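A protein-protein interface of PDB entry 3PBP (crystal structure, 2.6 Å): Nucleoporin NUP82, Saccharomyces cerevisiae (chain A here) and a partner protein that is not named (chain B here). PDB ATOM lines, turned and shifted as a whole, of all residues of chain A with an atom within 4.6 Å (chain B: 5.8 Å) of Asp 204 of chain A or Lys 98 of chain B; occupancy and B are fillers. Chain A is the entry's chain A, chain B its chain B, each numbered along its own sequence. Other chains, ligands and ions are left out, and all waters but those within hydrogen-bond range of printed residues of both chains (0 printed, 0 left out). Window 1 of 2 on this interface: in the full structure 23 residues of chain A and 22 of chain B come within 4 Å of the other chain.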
ATOM      1  N   CYS A 196     -16.109  -8.386 -27.503  1.00  0.00           N
ATOM      2  CA  CYS A 196     -15.056  -9.000 -28.309  1.00  0.00           C
ATOM      3  C   CYS A 196     -13.714  -8.489 -27.856  1.00  0.00           C
ATOM      4  O   CYS A 196     -13.537  -7.288 -27.699  1.00  0.00           O
ATOM      5  CB  CYS A 196     -15.216  -8.636 -29.783  1.00  0.00           C
ATOM      6  SG  CYS A 196     -16.806  -9.131 -30.463  1.00  0.00           S
ATOM      7  N   LEU A 197     -12.775  -9.398 -27.647  1.00  0.00           N
ATOM      8  CA  LEU A 197     -11.422  -9.028 -27.247  1.00  0.00           C
ATOM      9  C   LEU A 197     -10.520  -9.202 -28.474  1.00  0.00           C
ATOM     10  O   LEU A 197     -10.314 -10.321 -28.936  1.00  0.00           O
ATOM     11  CB  LEU A 197     -10.931  -9.936 -26.129  1.00  0.00           C
ATOM     12  CG  LEU A 197      -9.526  -9.628 -25.611  1.00  0.00           C
ATOM     13  CD1 LEU A 197      -9.556  -8.342 -24.806  1.00  0.00           C
ATOM     14  CD2 LEU A 197      -9.026 -10.769 -24.749  1.00  0.00           C
ATOM     15  N   ASN A 198      -9.992  -8.103 -29.008  1.00  0.00           N
ATOM     16  CA  ASN A 198      -9.130  -8.192 -30.182  1.00  0.00           C
ATOM     17  C   ASN A 198      -7.662  -7.898 -29.837  1.00  0.00           C
ATOM     18  O   ASN A 198      -7.353  -7.392 -28.752  1.00  0.00           O
ATOM     19  CB  ASN A 198      -9.647  -7.258 -31.286  1.00  0.00           C
ATOM     20  CG  ASN A 198      -8.989  -5.912 -31.263  1.00  0.00           C
ATOM     21  OD1 ASN A 198      -8.730  -5.351 -30.200  1.00  0.00           O
ATOM     22  ND2 ASN A 198      -8.723  -5.370 -32.439  1.00  0.00           N
ATOM     23  N   GLU A 201      -3.941  -4.107 -31.473  1.00  0.00           N
ATOM     24  CA  GLU A 201      -3.066  -3.177 -30.773  1.00  0.00           C
ATOM     25  C   GLU A 201      -2.746  -3.591 -29.355  1.00  0.00           C
ATOM     26  O   GLU A 201      -2.795  -2.772 -28.443  1.00  0.00           O
ATOM     27  CB  GLU A 201      -3.693  -1.786 -30.753  1.00  0.00           C
ATOM     28  CG  GLU A 201      -3.843  -1.159 -32.127  1.00  0.00           C
ATOM     29  CD  GLU A 201      -4.820   0.013 -32.134  1.00  0.00           C
ATOM     30  OE1 GLU A 201      -4.680   0.916 -31.275  1.00  0.00           O
ATOM     31  OE2 GLU A 201      -5.726   0.035 -33.002  1.00  0.00           O
ATOM     32  N   GLY A 203      -4.472  -5.411 -27.470  1.00  0.00           N
ATOM     33  CA  GLY A 203      -5.661  -5.821 -26.750  1.00  0.00           C
ATOM     34  C   GLY A 203      -6.655  -4.707 -26.493  1.00  0.00           C
ATOM     35  O   GLY A 203      -6.346  -3.700 -25.858  1.00  0.00           O
ATOM     36  N   ASP A 204      -7.863  -4.897 -26.998  1.00  0.00           N
ATOM     37  CA  ASP A 204      -8.928  -3.928 -26.821  1.00  0.00           C
ATOM     38  C   ASP A 204     -10.278  -4.630 -26.735  1.00  0.00           C
ATOM     39  O   ASP A 204     -10.388  -5.814 -27.038  1.00  0.00           O
ATOM     40  CB  ASP A 204      -8.918  -2.925 -27.971  1.00  0.00           C
ATOM     41  CG  ASP A 204      -7.917  -1.800 -27.747  1.00  0.00           C
ATOM     42  OD1 ASP A 204      -8.119  -1.002 -26.790  1.00  0.00           O
ATOM     43  OD2 ASP A 204      -6.930  -1.720 -28.526  1.00  0.00           O
ATOM     44  N   ILE A 205     -11.300  -3.902 -26.306  1.00  0.00           N
ATOM     45  CA  ILE A 205     -12.623  -4.478 -26.191  1.00  0.00           C
ATOM     46  C   ILE A 205     -13.620  -3.765 -27.105  1.00  0.00           C
ATOM     47  O   ILE A 205     -13.684  -2.546 -27.152  1.00  0.00           O
ATOM     48  CB  ILE A 205     -13.121  -4.418 -24.725  1.00  0.00           C
ATOM     49  CG1 ILE A 205     -12.196  -5.257 -23.847  1.00  0.00           C
ATOM     50  CG2 ILE A 205     -14.562  -4.891 -24.644  1.00  0.00           C
ATOM     51  CD1 ILE A 205     -12.488  -5.175 -22.388  1.00  0.00           C
ATOM     52  N   PHE A 206     -14.379  -4.542 -27.861  1.00  0.00           N
ATOM     53  CA  PHE A 206     -15.392  -3.972 -28.725  1.00  0.00           C
ATOM     54  C   PHE A 206     -16.683  -4.632 -28.293  1.00  0.00           C
ATOM     55  O   PHE A 206     -16.671  -5.558 -27.466  1.00  0.00           O
ATOM     56  CB  PHE A 206     -15.094  -4.267 -30.200  1.00  0.00           C
ATOM     57  CG  PHE A 206     -13.878  -3.548 -30.725  1.00  0.00           C
ATOM     58  CD1 PHE A 206     -12.591  -3.948 -30.351  1.00  0.00           C
ATOM     59  CD2 PHE A 206     -14.017  -2.437 -31.540  1.00  0.00           C
ATOM     60  CE1 PHE A 206     -11.463  -3.244 -30.783  1.00  0.00           C
ATOM     61  CE2 PHE A 206     -12.893  -1.727 -31.976  1.00  0.00           C
ATOM     62  CZ  PHE A 206     -11.616  -2.132 -31.593  1.00  0.00           C
ATOM     63  N   PRO A 284     -13.214   1.109 -29.975  1.00  0.00           N
ATOM     64  CA  PRO A 284     -12.832   0.395 -28.755  1.00  0.00           C
ATOM     65  C   PRO A 284     -13.332   1.043 -27.480  1.00  0.00           C
ATOM     66  O   PRO A 284     -13.555   2.249 -27.418  1.00  0.00           O
ATOM     67  CB  PRO A 284     -11.296   0.387 -28.797  1.00  0.00           C
ATOM     68  CG  PRO A 284     -10.917   1.251 -29.998  1.00  0.00           C
ATOM     69  CD  PRO A 284     -12.146   2.031 -30.375  1.00  0.00           C
ATOM     70  N   PHE A 285     -13.512   0.216 -26.461  1.00  0.00           N
ATOM     71  CA  PHE A 285     -13.938   0.699 -25.180  1.00  0.00           C
ATOM     72  C   PHE A 285     -12.725   1.348 -24.545  1.00  0.00           C
ATOM     73  O   PHE A 285     -11.582   0.972 -24.803  1.00  0.00           O
ATOM     74  CB  PHE A 285     -14.388  -0.448 -24.281  1.00  0.00           C
ATOM     75  CG  PHE A 285     -15.845  -0.752 -24.361  1.00  0.00           C
ATOM     76  CD1 PHE A 285     -16.400  -1.257 -25.526  1.00  0.00           C
ATOM     77  CD2 PHE A 285     -16.662  -0.540 -23.267  1.00  0.00           C
ATOM     78  CE1 PHE A 285     -17.750  -1.545 -25.599  1.00  0.00           C
ATOM     79  CE2 PHE A 285     -18.018  -0.822 -23.328  1.00  0.00           C
ATOM     80  CZ  PHE A 285     -18.565  -1.326 -24.495  1.00  0.00           C
ATOM     81  N   THR A 286     -12.991   2.328 -23.703  1.00  0.00           N
ATOM     82  CA  THR A 286     -11.958   3.020 -22.977  1.00  0.00           C
ATOM     83  C   THR A 286     -11.723   2.185 -21.714  1.00  0.00           C
ATOM     84  O   THR A 286     -12.678   1.780 -21.059  1.00  0.00           O
ATOM     85  CB  THR A 286     -12.463   4.410 -22.632  1.00  0.00           C
ATOM     86  OG1 THR A 286     -11.885   5.345 -23.537  1.00  0.00           O
ATOM     87  CG2 THR A 286     -12.128   4.785 -21.240  1.00  0.00           C
ATOM     88  N   ILE A 287     -10.475   1.875 -21.386  1.00  0.00           N
ATOM     89  CA  ILE A 287     -10.205   1.106 -20.164  1.00  0.00           C
ATOM     90  C   ILE A 287      -9.426   2.046 -19.258  1.00  0.00           C
ATOM     91  O   ILE A 287      -8.215   2.180 -19.387  1.00  0.00           O
ATOM     92  CB  ILE A 287      -9.357  -0.166 -20.435  1.00  0.00           C
ATOM     93  CG1 ILE A 287     -10.088  -1.093 -21.416  1.00  0.00           C
ATOM     94  CG2 ILE A 287      -9.098  -0.902 -19.129  1.00  0.00           C
ATOM     95  CD1 ILE A 287      -9.338  -2.360 -21.730  1.00  0.00           C
ATOM     96  N   PHE A 290      -5.785   2.448 -17.588  1.00  0.00           N
ATOM     97  CA  PHE A 290      -5.021   1.319 -18.104  1.00  0.00           C
ATOM     98  C   PHE A 290      -3.603   1.224 -17.547  1.00  0.00           C
ATOM     99  O   PHE A 290      -2.830   2.178 -17.634  1.00  0.00           O
ATOM    100  CB  PHE A 290      -4.942   1.376 -19.623  1.00  0.00           C
ATOM    101  CG  PHE A 290      -4.388   0.128 -20.225  1.00  0.00           C
ATOM    102  CD1 PHE A 290      -5.085  -1.076 -20.114  1.00  0.00           C
ATOM    103  CD2 PHE A 290      -3.155   0.133 -20.857  1.00  0.00           C
ATOM    104  CE1 PHE A 290      -4.557  -2.265 -20.620  1.00  0.00           C
ATOM    105  CE2 PHE A 290      -2.617  -1.051 -21.369  1.00  0.00           C
ATOM    106  CZ  PHE A 290      -3.323  -2.257 -21.248  1.00  0.00           C
ATOM    107  N   TYR A 295       1.114  -2.430 -21.691  1.00  0.00           N
ATOM    108  CA  TYR A 295       1.286  -1.975 -23.064  1.00  0.00           C
ATOM    109  C   TYR A 295       2.318  -2.872 -23.750  1.00  0.00           C
ATOM    110  O   TYR A 295       2.377  -2.939 -24.979  1.00  0.00           O
ATOM    111  CB  TYR A 295       1.744  -0.516 -23.096  1.00  0.00           C
ATOM    112  CG  TYR A 295       0.612   0.487 -23.057  1.00  0.00           C
ATOM    113  CD1 TYR A 295      -0.317   0.557 -24.095  1.00  0.00           C
ATOM    114  CD2 TYR A 295       0.464   1.370 -21.982  1.00  0.00           C
ATOM    115  CE1 TYR A 295      -1.365   1.478 -24.065  1.00  0.00           C
ATOM    116  CE2 TYR A 295      -0.581   2.292 -21.948  1.00  0.00           C
ATOM    117  CZ  TYR A 295      -1.490   2.338 -22.991  1.00  0.00           C
ATOM    118  OH  TYR A 295      -2.529   3.237 -22.957  1.00  0.00           O
ATOM    119  N   VAL B  96      -2.934   4.915 -29.762  1.00  0.00           N
ATOM    120  CA  VAL B  96      -3.921   5.515 -28.881  1.00  0.00           C
ATOM    121  C   VAL B  96      -3.809   5.105 -27.420  1.00  0.00           C
ATOM    122  O   VAL B  96      -3.493   3.954 -27.101  1.00  0.00           O
ATOM    123  CB  VAL B  96      -5.343   5.218 -29.374  1.00  0.00           C
ATOM    124  CG1 VAL B  96      -6.357   5.758 -28.386  1.00  0.00           C
ATOM    125  CG2 VAL B  96      -5.557   5.852 -30.733  1.00  0.00           C
ATOM    126  N   ASP B  97      -4.059   6.068 -26.537  1.00  0.00           N
ATOM    127  CA  ASP B  97      -4.022   5.818 -25.104  1.00  0.00           C
ATOM    128  C   ASP B  97      -5.323   5.105 -24.748  1.00  0.00           C
ATOM    129  O   ASP B  97      -6.405   5.657 -24.932  1.00  0.00           O
ATOM    130  CB  ASP B  97      -3.895   7.143 -24.345  1.00  0.00           C
ATOM    131  CG  ASP B  97      -4.186   7.007 -22.857  1.00  0.00           C
ATOM    132  OD1 ASP B  97      -3.745   6.014 -22.220  1.00  0.00           O
ATOM    133  OD2 ASP B  97      -4.849   7.918 -22.324  1.00  0.00           O
ATOM    134  N   LYS B  98      -5.204   3.879 -24.243  1.00  0.00           N
ATOM    135  CA  LYS B  98      -6.356   3.060 -23.900  1.00  0.00           C
ATOM    136  C   LYS B  98      -7.365   3.587 -22.879  1.00  0.00           C
ATOM    137  O   LYS B  98      -8.515   3.147 -22.866  1.00  0.00           O
ATOM    138  CB  LYS B  98      -5.892   1.673 -23.459  1.00  0.00           C
ATOM    139  CG  LYS B  98      -5.310   0.842 -24.571  1.00  0.00           C
ATOM    140  CD  LYS B  98      -5.058  -0.578 -24.111  1.00  0.00           C
ATOM    141  CE  LYS B  98      -4.245  -1.328 -25.147  1.00  0.00           C
ATOM    142  NZ  LYS B  98      -4.892  -1.308 -26.490  1.00  0.00           N
ATOM    143  N   SER B  99      -6.967   4.516 -22.025  1.00  0.00           N
ATOM    144  CA  SER B  99      -7.899   5.018 -21.026  1.00  0.00           C
ATOM    145  C   SER B  99      -8.581   6.305 -21.453  1.00  0.00           C
ATOM    146  O   SER B  99      -9.496   6.787 -20.782  1.00  0.00           O
ATOM    147  CB  SER B  99      -7.169   5.229 -19.702  1.00  0.00           C
ATOM    148  OG  SER B  99      -5.962   5.928 -19.909  1.00  0.00           O
ATOM    149  N   THR B 100      -8.162   6.829 -22.594  1.00  0.00           N
ATOM    150  CA  THR B 100      -8.691   8.088 -23.091  1.00  0.00           C
ATOM    151  C   THR B 100      -9.172   7.991 -24.522  1.00  0.00           C
ATOM    152  O   THR B 100     -10.104   8.689 -24.934  1.00  0.00           O
ATOM    153  CB  THR B 100      -7.602   9.179 -23.029  1.00  0.00           C
ATOM    154  OG1 THR B 100      -7.298   9.477 -21.659  1.00  0.00           O
ATOM    155  CG2 THR B 100      -8.063  10.427 -23.719  1.00  0.00           C
ATOM    156  N   ARG B 101      -8.517   7.123 -25.277  1.00  0.00           N
ATOM    157  CA  ARG B 101      -8.819   6.934 -26.687  1.00  0.00           C
ATOM    158  C   ARG B 101      -8.240   8.118 -27.495  1.00  0.00           C
ATOM    159  O   ARG B 101      -8.545   8.297 -28.676  1.00  0.00           O
ATOM    160  CB  ARG B 101     -10.330   6.802 -26.914  1.00  0.00           C
ATOM    161  CG  ARG B 101     -10.665   6.169 -28.266  1.00  0.00           C
ATOM    162  CD  ARG B 101     -12.163   6.055 -28.523  1.00  0.00           C
ATOM    163  NE  ARG B 101     -12.821   5.173 -27.564  1.00  0.00           N
ATOM    164  CZ  ARG B 101     -13.694   5.584 -26.648  1.00  0.00           C
ATOM    165  NH1 ARG B 101     -14.030   6.867 -26.565  1.00  0.00           N
ATOM    166  NH2 ARG B 101     -14.223   4.710 -25.799  1.00  0.00           N
ATOM    167  N   ILE B 104      -1.539   9.350 -28.920  1.00  0.00           N
ATOM    168  CA  ILE B 104      -0.305   9.515 -28.159  1.00  0.00           C
ATOM    169  C   ILE B 104       0.751   9.997 -29.146  1.00  0.00           C
ATOM    170  O   ILE B 104       1.292   9.213 -29.930  1.00  0.00           O
ATOM    171  CB  ILE B 104       0.146   8.189 -27.532  1.00  0.00           C
ATOM    172  CG1 ILE B 104      -0.863   7.761 -26.469  1.00  0.00           C
ATOM    173  CG2 ILE B 104       1.546   8.337 -26.937  1.00  0.00           C
ATOM    174  CD1 ILE B 104      -0.572   6.407 -25.878  1.00  0.00           C
ATOM    175  N   LEU B 111       4.052   2.342 -26.746  1.00  0.00           N
ATOM    176  CA  LEU B 111       3.182   2.060 -27.878  1.00  0.00           C
ATOM    177  C   LEU B 111       3.817   2.348 -29.233  1.00  0.00           C
ATOM    178  O   LEU B 111       3.512   1.675 -30.217  1.00  0.00           O
ATOM    179  CB  LEU B 111       1.868   2.836 -27.749  1.00  0.00           C
ATOM    180  CG  LEU B 111       0.760   2.189 -26.907  1.00  0.00           C
ATOM    181  CD1 LEU B 111      -0.468   3.089 -26.911  1.00  0.00           C
ATOM    182  CD2 LEU B 111       0.410   0.809 -27.473  1.00  0.00           C
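NH2 of Arg 101 of chain B touches C of Phe 285 of chain A, at 3.9 Å. O of Lys 98 of chain B touches CA of Thr 286 of chain A, at 3.4 Å. Ser 99 of chain B touches Thr 286 of chain A. Thr 100 of chain B touches Thr 286 of chain A. CB of Ser 99 of chain B touches O of Ile 287 of chain A (3.2 Å). Phe 290 of chain A touches Lys 98 of chain B (CE2 to CD, 3.7 Å). Phe 290 of chain A touches Ser 99 of chain B. Tyr 295 of chain A touches Leu 111 of chain B (CE1 to CD1, 3.4 Å).
Of chain B, only Lys 98 (2.9 Å) comes within 4 Å of Asp 204 of chain A. Printed residues of chain B within 4 Å of Pro 284 of chain A: Arg 101. Of the printed residues of chain B, Thr 286 of chain A touches Lys 98, Ser 99, Thr 100 and Arg 101. Printed residues of chain B within 4 Å of Ile 287 of chain A: Lys 98 (2.8 Å) and Ser 99 (3.2 Å). Printed residues of chain B within 4 Å of Tyr 295 of chain A: Asp 97 (3.1 Å), Lys 98 (3.0 Å) and Leu 111 (3.4 Å). Val 96 of chain B touches none of the printed residues of chain A. Lys 98 of chain B touches just these residues of chain A: Glu 201, Gly 203, Asp 204, Thr 286, Ile 287, Phe 290 and Tyr 295. Ile 104 of chain B touches none of the printed residues of chain A. The nearest residue of chain A that does not touch Lys 98 of chain B is Phe 285 of chain A (4.2 Å).
OD2 of Asp 97 of chain B lies within hydrogen-bond range of OG1 of Thr 100 of chain B (3.0 Å). OD1 of Asp 97 of chain B sits at hydrogen-bond distance from OG of Ser 99 of chain B (3.2 Å). The backbone carbonyl oxygen (O) of Ile 205 of chain A is in hydrogen-bond range of the backbone NH (N) of Phe 285 of chain A (2.9 Å). The backbone NH (N) of Asn 198 of chain A sits at hydrogen-bond distance from the backbone carbonyl oxygen (O) of Asp 204 of chain A (3.0 Å).
Of the 8 printed residues of chain B, 6 touch a printed residue of chain A.
The side-chain hydroxyl (OH) of Tyr 295 of chain A is in hydrogen-bond range of the backbone NH (N) of Lys 98 of chain B, at 3.0 Å. NZ of Lys 98 of chain B lies within hydrogen-bond range of O of Glu 201 of chain A (3.2 Å). NE of Arg 101 of chain B sits at hydrogen-bond distance from O of Pro 284 of chain A, 3.0 Å away. The backbone carbonyl oxygen (O) of Gly 203 of chain A sits at hydrogen-bond distance from the side-chain amino group (NZ) of Lys 98 of chain B (2.9 Å). O of Lys 98 of chain B is in hydrogen-bond range of N of Ile 287 of chain A (2.8 Å). The side-chain carboxylate of Asp 204 of chain A is in salt-bridge range of the side-chain amino group of Lys 98 of chain B (2.9 Å). OG1 of Thr 286 of chain A lies within hydrogen-bond range of NH2 of Arg 101 of chain B (3.3 Å). The side-chain hydroxyl of Tyr 295 of chain A is in hydrogen-bond range of the side-chain carboxylate of Asp 97 of chain B (3.1 Å).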
